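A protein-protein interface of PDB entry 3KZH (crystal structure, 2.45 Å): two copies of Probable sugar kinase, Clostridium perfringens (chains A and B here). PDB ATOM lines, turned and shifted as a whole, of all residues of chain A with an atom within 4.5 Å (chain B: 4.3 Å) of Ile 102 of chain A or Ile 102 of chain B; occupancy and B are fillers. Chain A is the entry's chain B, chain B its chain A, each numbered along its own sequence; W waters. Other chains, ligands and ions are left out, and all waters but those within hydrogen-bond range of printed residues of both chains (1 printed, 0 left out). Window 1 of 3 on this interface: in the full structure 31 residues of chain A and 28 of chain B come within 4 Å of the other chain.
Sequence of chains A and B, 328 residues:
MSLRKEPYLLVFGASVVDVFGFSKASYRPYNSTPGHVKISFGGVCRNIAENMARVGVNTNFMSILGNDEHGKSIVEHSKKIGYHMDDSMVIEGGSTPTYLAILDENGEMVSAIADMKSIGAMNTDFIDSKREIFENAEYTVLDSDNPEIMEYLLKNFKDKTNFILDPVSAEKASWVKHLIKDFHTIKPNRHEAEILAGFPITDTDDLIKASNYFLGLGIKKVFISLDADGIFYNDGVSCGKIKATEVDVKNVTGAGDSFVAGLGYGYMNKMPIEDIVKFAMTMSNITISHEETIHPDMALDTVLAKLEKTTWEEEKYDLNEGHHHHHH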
ATOM      1  N   GLY A  21     -21.507   3.791 -22.933  1.00  0.00           N
ATOM      2  CA  GLY A  21     -20.543   4.809 -22.573  1.00  0.00           C
ATOM      3  C   GLY A  21     -19.307   4.102 -22.056  1.00  0.00           C
ATOM      4  O   GLY A  21     -19.313   3.597 -20.932  1.00  0.00           O
ATOM      5  N   TYR A  27     -12.604   4.896 -13.477  1.00  0.00           N
ATOM      6  CA  TYR A  27     -13.997   5.094 -13.106  1.00  0.00           C
ATOM      7  C   TYR A  27     -14.225   5.554 -11.669  1.00  0.00           C
ATOM      8  O   TYR A  27     -13.659   5.009 -10.721  1.00  0.00           O
ATOM      9  CB  TYR A  27     -14.848   3.853 -13.422  1.00  0.00           C
ATOM     10  CG  TYR A  27     -16.334   4.120 -13.309  1.00  0.00           C
ATOM     11  CD1 TYR A  27     -17.010   4.890 -14.284  1.00  0.00           C
ATOM     12  CD2 TYR A  27     -17.049   3.720 -12.160  1.00  0.00           C
ATOM     13  CE1 TYR A  27     -18.367   5.264 -14.106  1.00  0.00           C
ATOM     14  CE2 TYR A  27     -18.391   4.095 -11.970  1.00  0.00           C
ATOM     15  CZ  TYR A  27     -19.041   4.861 -12.941  1.00  0.00           C
ATOM     16  OH  TYR A  27     -20.343   5.216 -12.717  1.00  0.00           O
ATOM     17  N   LEU A 100     -29.306   1.794 -21.742  1.00  0.00           N
ATOM     18  CA  LEU A 100     -28.185   2.694 -21.444  1.00  0.00           C
ATOM     19  C   LEU A 100     -27.254   1.975 -20.504  1.00  0.00           C
ATOM     20  O   LEU A 100     -27.700   1.468 -19.483  1.00  0.00           O
ATOM     21  CB  LEU A 100     -28.625   3.966 -20.720  1.00  0.00           C
ATOM     22  CG  LEU A 100     -29.635   4.971 -21.247  1.00  0.00           C
ATOM     23  CD1 LEU A 100     -29.488   6.225 -20.434  1.00  0.00           C
ATOM     24  CD2 LEU A 100     -29.431   5.289 -22.697  1.00  0.00           C
ATOM     25  N   ALA A 101     -25.964   1.967 -20.831  1.00  0.00           N
ATOM     26  CA  ALA A 101     -24.962   1.313 -19.999  1.00  0.00           C
ATOM     27  C   ALA A 101     -23.640   2.063 -19.952  1.00  0.00           C
ATOM     28  O   ALA A 101     -23.071   2.416 -20.986  1.00  0.00           O
ATOM     29  CB  ALA A 101     -24.743  -0.121 -20.453  1.00  0.00           C
ATOM     30  N   ILE A 102     -23.176   2.317 -18.732  1.00  0.00           N
ATOM     31  CA  ILE A 102     -21.915   3.006 -18.491  1.00  0.00           C
ATOM     32  C   ILE A 102     -20.890   1.964 -18.033  1.00  0.00           C
ATOM     33  O   ILE A 102     -20.960   1.432 -16.917  1.00  0.00           O
ATOM     34  CB  ILE A 102     -22.117   4.187 -17.483  1.00  0.00           C
ATOM     35  CG1 ILE A 102     -22.871   5.314 -18.201  1.00  0.00           C
ATOM     36  CG2 ILE A 102     -20.777   4.713 -16.940  1.00  0.00           C
ATOM     37  CD1 ILE A 102     -23.498   6.335 -17.323  1.00  0.00           C
ATOM     38  N   LEU A 103     -19.987   1.642 -18.957  1.00  0.00           N
ATOM     39  CA  LEU A 103     -18.918   0.666 -18.757  1.00  0.00           C
ATOM     40  C   LEU A 103     -17.621   1.294 -18.244  1.00  0.00           C
ATOM     41  O   LEU A 103     -17.315   2.445 -18.571  1.00  0.00           O
ATOM     42  CB  LEU A 103     -18.651  -0.088 -20.067  1.00  0.00           C
ATOM     43  CG  LEU A 103     -19.638  -1.164 -20.543  1.00  0.00           C
ATOM     44  CD1 LEU A 103     -20.993  -0.591 -20.877  1.00  0.00           C
ATOM     45  CD2 LEU A 103     -19.088  -1.859 -21.757  1.00  0.00           C
ATOM     46  N   ASP A 104     -16.865   0.534 -17.444  1.00  0.00           N
ATOM     47  CA  ASP A 104     -15.597   1.012 -16.895  1.00  0.00           C
ATOM     48  C   ASP A 104     -14.419   0.873 -17.870  1.00  0.00           C
ATOM     49  O   ASP A 104     -14.619   0.607 -19.056  1.00  0.00           O
ATOM     50  CB  ASP A 104     -15.288   0.389 -15.508  1.00  0.00           C
ATOM     51  CG  ASP A 104     -15.111  -1.150 -15.523  1.00  0.00           C
ATOM     52  OD1 ASP A 104     -14.812  -1.773 -16.572  1.00  0.00           O
ATOM     53  OD2 ASP A 104     -15.246  -1.739 -14.429  1.00  0.00           O
ATOM     54  N   MET A 109     -19.709  -3.335 -17.097  1.00  0.00           N
ATOM     55  CA  MET A 109     -20.664  -2.301 -16.677  1.00  0.00           C
ATOM     56  C   MET A 109     -20.767  -2.028 -15.175  1.00  0.00           C
ATOM     57  O   MET A 109     -20.714  -2.945 -14.356  1.00  0.00           O
ATOM     58  CB  MET A 109     -22.049  -2.505 -17.334  1.00  0.00           C
ATOM     59  CG  MET A 109     -23.050  -3.367 -16.593  1.00  0.00           C
ATOM     60  SD  MET A 109     -24.214  -2.415 -15.353  1.00  0.00           S
ATOM     61  CE  MET A 109     -25.623  -3.749 -15.533  1.00  0.00           C
ATOM     62  N   VAL A 110     -20.919  -0.745 -14.847  1.00  0.00           N
ATOM     63  CA  VAL A 110     -21.043  -0.255 -13.472  1.00  0.00           C
ATOM     64  C   VAL A 110     -22.421   0.397 -13.216  1.00  0.00           C
ATOM     65  O   VAL A 110     -22.828   0.563 -12.061  1.00  0.00           O
ATOM     66  CB  VAL A 110     -19.927   0.781 -13.129  1.00  0.00           C
ATOM     67  CG1 VAL A 110     -19.804   0.944 -11.613  1.00  0.00           C
ATOM     68  CG2 VAL A 110     -18.585   0.377 -13.716  1.00  0.00           C
ATOM     69  N   SER A 111     -23.112   0.783 -14.292  1.00  0.00           N
ATOM     70  CA  SER A 111     -24.440   1.407 -14.214  1.00  0.00           C
ATOM     71  C   SER A 111     -25.233   1.138 -15.486  1.00  0.00           C
ATOM     72  O   SER A 111     -24.652   1.100 -16.573  1.00  0.00           O
ATOM     73  CB  SER A 111     -24.308   2.907 -14.025  1.00  0.00           C
ATOM     74  OG  SER A 111     -25.536   3.486 -13.614  1.00  0.00           O
ATOM     75  N   ALA A 112     -26.553   0.976 -15.348  1.00  0.00           N
ATOM     76  CA  ALA A 112     -27.431   0.683 -16.491  1.00  0.00           C
ATOM     77  C   ALA A 112     -28.922   0.959 -16.321  1.00  0.00           C
ATOM     78  O   ALA A 112     -29.483   0.784 -15.237  1.00  0.00           O
ATOM     79  CB  ALA A 112     -27.226  -0.759 -16.970  1.00  0.00           C
ATOM     80  N   ILE A 113     -29.540   1.407 -17.415  1.00  0.00           N
ATOM     81  CA  ILE A 113     -30.969   1.727 -17.481  1.00  0.00           C
ATOM     82  C   ILE A 113     -31.606   0.986 -18.660  1.00  0.00           C
ATOM     83  O   ILE A 113     -31.191   1.161 -19.810  1.00  0.00           O
ATOM     84  CB  ILE A 113     -31.240   3.282 -17.645  1.00  0.00           C
ATOM     85  CG1 ILE A 113     -30.872   4.069 -16.381  1.00  0.00           C
ATOM     86  CG2 ILE A 113     -32.704   3.577 -18.043  1.00  0.00           C
ATOM     87  CD1 ILE A 113     -31.804   3.930 -15.180  1.00  0.00           C
ATOM     88  N   GLY B  21     -30.831   8.963 -18.349  1.00  0.00           N
ATOM     89  CA  GLY B  21     -31.573   7.789 -17.916  1.00  0.00           C
ATOM     90  C   GLY B  21     -32.076   7.997 -16.503  1.00  0.00           C
ATOM     91  O   GLY B  21     -31.277   8.097 -15.576  1.00  0.00           O
ATOM     92  N   TYR B  27     -32.211   2.435  -7.482  1.00  0.00           N
ATOM     93  CA  TYR B  27     -30.908   2.281  -8.132  1.00  0.00           C
ATOM     94  C   TYR B  27     -29.922   1.475  -7.283  1.00  0.00           C
ATOM     95  O   TYR B  27     -29.887   1.588  -6.054  1.00  0.00           O
ATOM     96  CB  TYR B  27     -30.306   3.655  -8.505  1.00  0.00           C
ATOM     97  CG  TYR B  27     -28.937   3.580  -9.164  1.00  0.00           C
ATOM     98  CD1 TYR B  27     -28.808   3.166 -10.503  1.00  0.00           C
ATOM     99  CD2 TYR B  27     -27.754   3.803  -8.415  1.00  0.00           C
ATOM    100  CE1 TYR B  27     -27.532   2.961 -11.090  1.00  0.00           C
ATOM    101  CE2 TYR B  27     -26.475   3.594  -8.983  1.00  0.00           C
ATOM    102  CZ  TYR B  27     -26.375   3.176 -10.320  1.00  0.00           C
ATOM    103  OH  TYR B  27     -25.139   2.978 -10.887  1.00  0.00           O
ATOM    104  N   LEU B 100     -23.781  11.434 -21.494  1.00  0.00           N
ATOM    105  CA  LEU B 100     -24.603  10.299 -21.085  1.00  0.00           C
ATOM    106  C   LEU B 100     -24.627  10.220 -19.559  1.00  0.00           C
ATOM    107  O   LEU B 100     -23.596  10.002 -18.943  1.00  0.00           O
ATOM    108  CB  LEU B 100     -24.043   9.009 -21.701  1.00  0.00           C
ATOM    109  CG  LEU B 100     -24.565   7.617 -21.311  1.00  0.00           C
ATOM    110  CD1 LEU B 100     -26.067   7.481 -21.553  1.00  0.00           C
ATOM    111  CD2 LEU B 100     -23.808   6.582 -22.112  1.00  0.00           C
ATOM    112  N   ALA B 101     -25.802  10.406 -18.961  1.00  0.00           N
ATOM    113  CA  ALA B 101     -25.934  10.351 -17.506  1.00  0.00           C
ATOM    114  C   ALA B 101     -27.083   9.517 -16.995  1.00  0.00           C
ATOM    115  O   ALA B 101     -28.183   9.556 -17.538  1.00  0.00           O
ATOM    116  CB  ALA B 101     -26.034  11.742 -16.922  1.00  0.00           C
ATOM    117  N   ILE B 102     -26.816   8.776 -15.922  1.00  0.00           N
ATOM    118  CA  ILE B 102     -27.823   7.938 -15.279  1.00  0.00           C
ATOM    119  C   ILE B 102     -28.159   8.547 -13.915  1.00  0.00           C
ATOM    120  O   ILE B 102     -27.270   8.793 -13.097  1.00  0.00           O
ATOM    121  CB  ILE B 102     -27.354   6.447 -15.186  1.00  0.00           C
ATOM    122  CG1 ILE B 102     -27.398   5.828 -16.588  1.00  0.00           C
ATOM    123  CG2 ILE B 102     -28.230   5.644 -14.210  1.00  0.00           C
ATOM    124  CD1 ILE B 102     -26.731   4.503 -16.732  1.00  0.00           C
ATOM    125  N   LEU B 103     -29.442   8.850 -13.728  1.00  0.00           N
ATOM    126  CA  LEU B 103     -29.955   9.434 -12.490  1.00  0.00           C
ATOM    127  C   LEU B 103     -30.711   8.389 -11.670  1.00  0.00           C
ATOM    128  O   LEU B 103     -31.270   7.439 -12.235  1.00  0.00           O
ATOM    129  CB  LEU B 103     -30.893  10.622 -12.776  1.00  0.00           C
ATOM    130  CG  LEU B 103     -30.563  11.820 -13.684  1.00  0.00           C
ATOM    131  CD1 LEU B 103     -29.158  12.329 -13.474  1.00  0.00           C
ATOM    132  CD2 LEU B 103     -30.748  11.433 -15.134  1.00  0.00           C
ATOM    133  N   GLU B 108     -30.739  12.331  -8.612  1.00  0.00           N
ATOM    134  CA  GLU B 108     -29.315  12.631  -8.500  1.00  0.00           C
ATOM    135  C   GLU B 108     -28.458  11.774  -9.415  1.00  0.00           C
ATOM    136  O   GLU B 108     -28.729  10.583  -9.597  1.00  0.00           O
ATOM    137  CB  GLU B 108     -28.841  12.459  -7.058  1.00  0.00           C
ATOM    138  CG  GLU B 108     -29.394  13.498  -6.105  1.00  0.00           C
ATOM    139  CD  GLU B 108     -28.361  13.977  -5.108  1.00  0.00           C
ATOM    140  OE1 GLU B 108     -27.335  14.554  -5.538  1.00  0.00           O
ATOM    141  OE2 GLU B 108     -28.580  13.782  -3.894  1.00  0.00           O
ATOM    142  N   MET B 109     -27.412  12.387  -9.972  1.00  0.00           N
ATOM    143  CA  MET B 109     -26.489  11.691 -10.862  1.00  0.00           C
ATOM    144  C   MET B 109     -25.619  10.732 -10.053  1.00  0.00           C
ATOM    145  O   MET B 109     -24.953  11.117  -9.081  1.00  0.00           O
ATOM    146  CB  MET B 109     -25.684  12.688 -11.741  1.00  0.00           C
ATOM    147  CG  MET B 109     -24.217  12.947 -11.389  1.00  0.00           C
ATOM    148  SD  MET B 109     -23.008  11.691 -12.245  1.00  0.00           S
ATOM    149  CE  MET B 109     -21.942  13.150 -13.006  1.00  0.00           C
ATOM    150  N   VAL B 110     -25.731   9.462 -10.418  1.00  0.00           N
ATOM    151  CA  VAL B 110     -24.995   8.389  -9.776  1.00  0.00           C
ATOM    152  C   VAL B 110     -23.959   7.800 -10.722  1.00  0.00           C
ATOM    153  O   VAL B 110     -23.136   6.977 -10.310  1.00  0.00           O
ATOM    154  CB  VAL B 110     -25.949   7.273  -9.288  1.00  0.00           C
ATOM    155  CG1 VAL B 110     -26.669   7.702  -8.032  1.00  0.00           C
ATOM    156  CG2 VAL B 110     -26.969   6.916 -10.381  1.00  0.00           C
ATOM    157  N   SER B 111     -24.009   8.237 -11.984  1.00  0.00           N
ATOM    158  CA  SER B 111     -23.098   7.765 -13.037  1.00  0.00           C
ATOM    159  C   SER B 111     -23.200   8.639 -14.295  1.00  0.00           C
ATOM    160  O   SER B 111     -24.286   9.138 -14.613  1.00  0.00           O
ATOM    161  CB  SER B 111     -23.457   6.325 -13.399  1.00  0.00           C
ATOM    162  OG  SER B 111     -22.456   5.688 -14.164  1.00  0.00           O
ATOM    163  N   ALA B 112     -22.070   8.813 -14.998  1.00  0.00           N
ATOM    164  CA  ALA B 112     -21.994   9.612 -16.234  1.00  0.00           C
ATOM    165  C   ALA B 112     -20.735   9.457 -17.078  1.00  0.00           C
ATOM    166  O   ALA B 112     -19.655   9.174 -16.559  1.00  0.00           O
ATOM    167  CB  ALA B 112     -22.220  11.096 -15.954  1.00  0.00           C
ATOM    168  N   ILE B 113     -20.910   9.651 -18.388  1.00  0.00           N
ATOM    169  CA  ILE B 113     -19.844   9.600 -19.393  1.00  0.00           C
ATOM    170  C   ILE B 113     -19.910  10.901 -20.203  1.00  0.00           C
ATOM    171  O   ILE B 113     -20.954  11.223 -20.786  1.00  0.00           O
ATOM    172  CB  ILE B 113     -19.974   8.350 -20.357  1.00  0.00           C
ATOM    173  CG1 ILE B 113     -19.587   7.055 -19.627  1.00  0.00           C
ATOM    174  CG2 ILE B 113     -19.098   8.504 -21.619  1.00  0.00           C
ATOM    175  CD1 ILE B 113     -18.129   6.948 -19.157  1.00  0.00           C
HETATM  176  O   HOH W   1     -19.631   8.398 -13.448  1.00  0.00           O
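The side-chain hydroxyl (OH) of Tyr 27 of chain B is in hydrogen-bond range of the side-chain hydroxyl (OG) of Ser 111 of chain A (2.8 Å).
The side-chain hydroxyl (OH) of Tyr 27 of chain A is in hydrogen-bond range of the side-chain hydroxyl (OG) of Ser 111 of chain B (2.6 Å).
The backbone carbonyl oxygen (O) of Gly 21 of chain B sits at hydrogen-bond distance from the backbone NH (N) of Leu 103 of chain B (2.7 Å).
N of Val 110 of chain B lies within hydrogen-bond range of O of Ile 102 of chain B (3.2 Å).
The backbone NH of Ile 102 of chain B sits at hydrogen-bond distance from the backbone carbonyl oxygen of Ser 111 of chain B, 2.9 Å away.
The backbone carbonyl oxygen (O) of Gly 21 of chain A sits at hydrogen-bond distance from the backbone NH (N) of Leu 103 of chain A, 2.9 Å away.
The backbone carbonyl oxygen (O) of Ile 102 of chain A lies within hydrogen-bond range of the backbone NH (N) of Val 110 of chain A, 3.0 Å away.
The backbone NH (N) of Ser 111 of chain A is in hydrogen-bond range of the side-chain sulfur (SD) of Met 109 of chain A.
O of Gly 21 of chain A touches CG1 of Ile 113 of chain B, 3.7 Å away.
Gly 21 of chain B touches Leu 100 of chain A (CA to CD1, 3.6 Å).
CD1 of Leu 100 of chain A touches CD1 of Leu 100 of chain B, at 3.8 Å.
Ile 102 of chain A touches Ile 102 of chain B (CD1 to CD1, 3.8 Å).
Ile 102 of chain A touches Ser 111 of chain B.
Ile 102 of chain A touches Ile 113 of chain B.
O of Val 110 of chain A touches OH of Tyr 27 of chain B, at 3.5 Å.
CB of Ser 111 of chain A touches OG of Ser 111 of chain B, 3.3 Å away.
Ala 112 of chain A touches Ile 102 of chain B.
Ile 113 of chain A touches Ile 102 of chain B.
Printed residues of chain B within 4 Å of Ile 102 of chain A: Ile 102 (3.8 Å), Ser 111 (3.4 Å), Ala 112 (3.7 Å) and Ile 113 (3.8 Å).
Of the printed residues of chain A, Ile 102 of chain B touches Ile 102, Ser 111, Ala 112 and Ile 113.
Printed residues of chain A within 4 Å of Ile 113 of chain B: Gly 21 and Ile 102.
Of the printed residues of chain B, Tyr 27 of chain A touches Ser 111.
Of the printed residues of chain A, Leu 100 of chain B touches Gly 21 (3.7 Å) and Leu 100 (3.8 Å).
Leu 103 of chain B touches none of the printed residues of chain A.
The nearest printed residue of chain B that does not touch Ile 102 of chain A is Leu 100 of chain B (4.01 Å).
The nearest printed residue of chain B that does not touch Leu 100 of chain A is Ile 102 of chain B (4.2 Å).
Hydrophobic or aromatic side chains of chain B that line the printed part of chain A: Tyr 27, Leu 100, Ile 102 and Ile 113.
Among the printed residues, 15 pairs touch across the chains.
Among the printed residues, no Asp or Glu carboxylate lies within 4 Å of a Lys or Arg side-chain nitrogen of the other chain.
Tyr 27 of chain A touches Ser 111 of chain B, and with the chains exchanged Ser 111 of chain A touches Tyr 27 of chain B.
Ile 102 of chain A touches its own counterpart, Ile 102 of chain B.
Ile 102 of chain A touches Ser 111 of chain B, and with the chains exchanged Ser 111 of chain A touches Ile 102 of chain B.
Val 110 of chain A touches Tyr 27 of chain B, but with the chains exchanged Tyr 27 of chain A does not touch Val 110 of chain B (4.1 Å).
Positions printed for both chains: 21, 27, 100, 101, 102, 103, 109, 110, 111, 112 and 113.
Of the 15 pairs that touch across the chains among the printed residues, 13 have their exchanged pair printed and touching as well.
Water W1 lies within hydrogen-bond range of the backbone NH (N) of Ala 112 of chain B and the side-chain hydroxyl (OH) of Tyr 27 of chain A.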
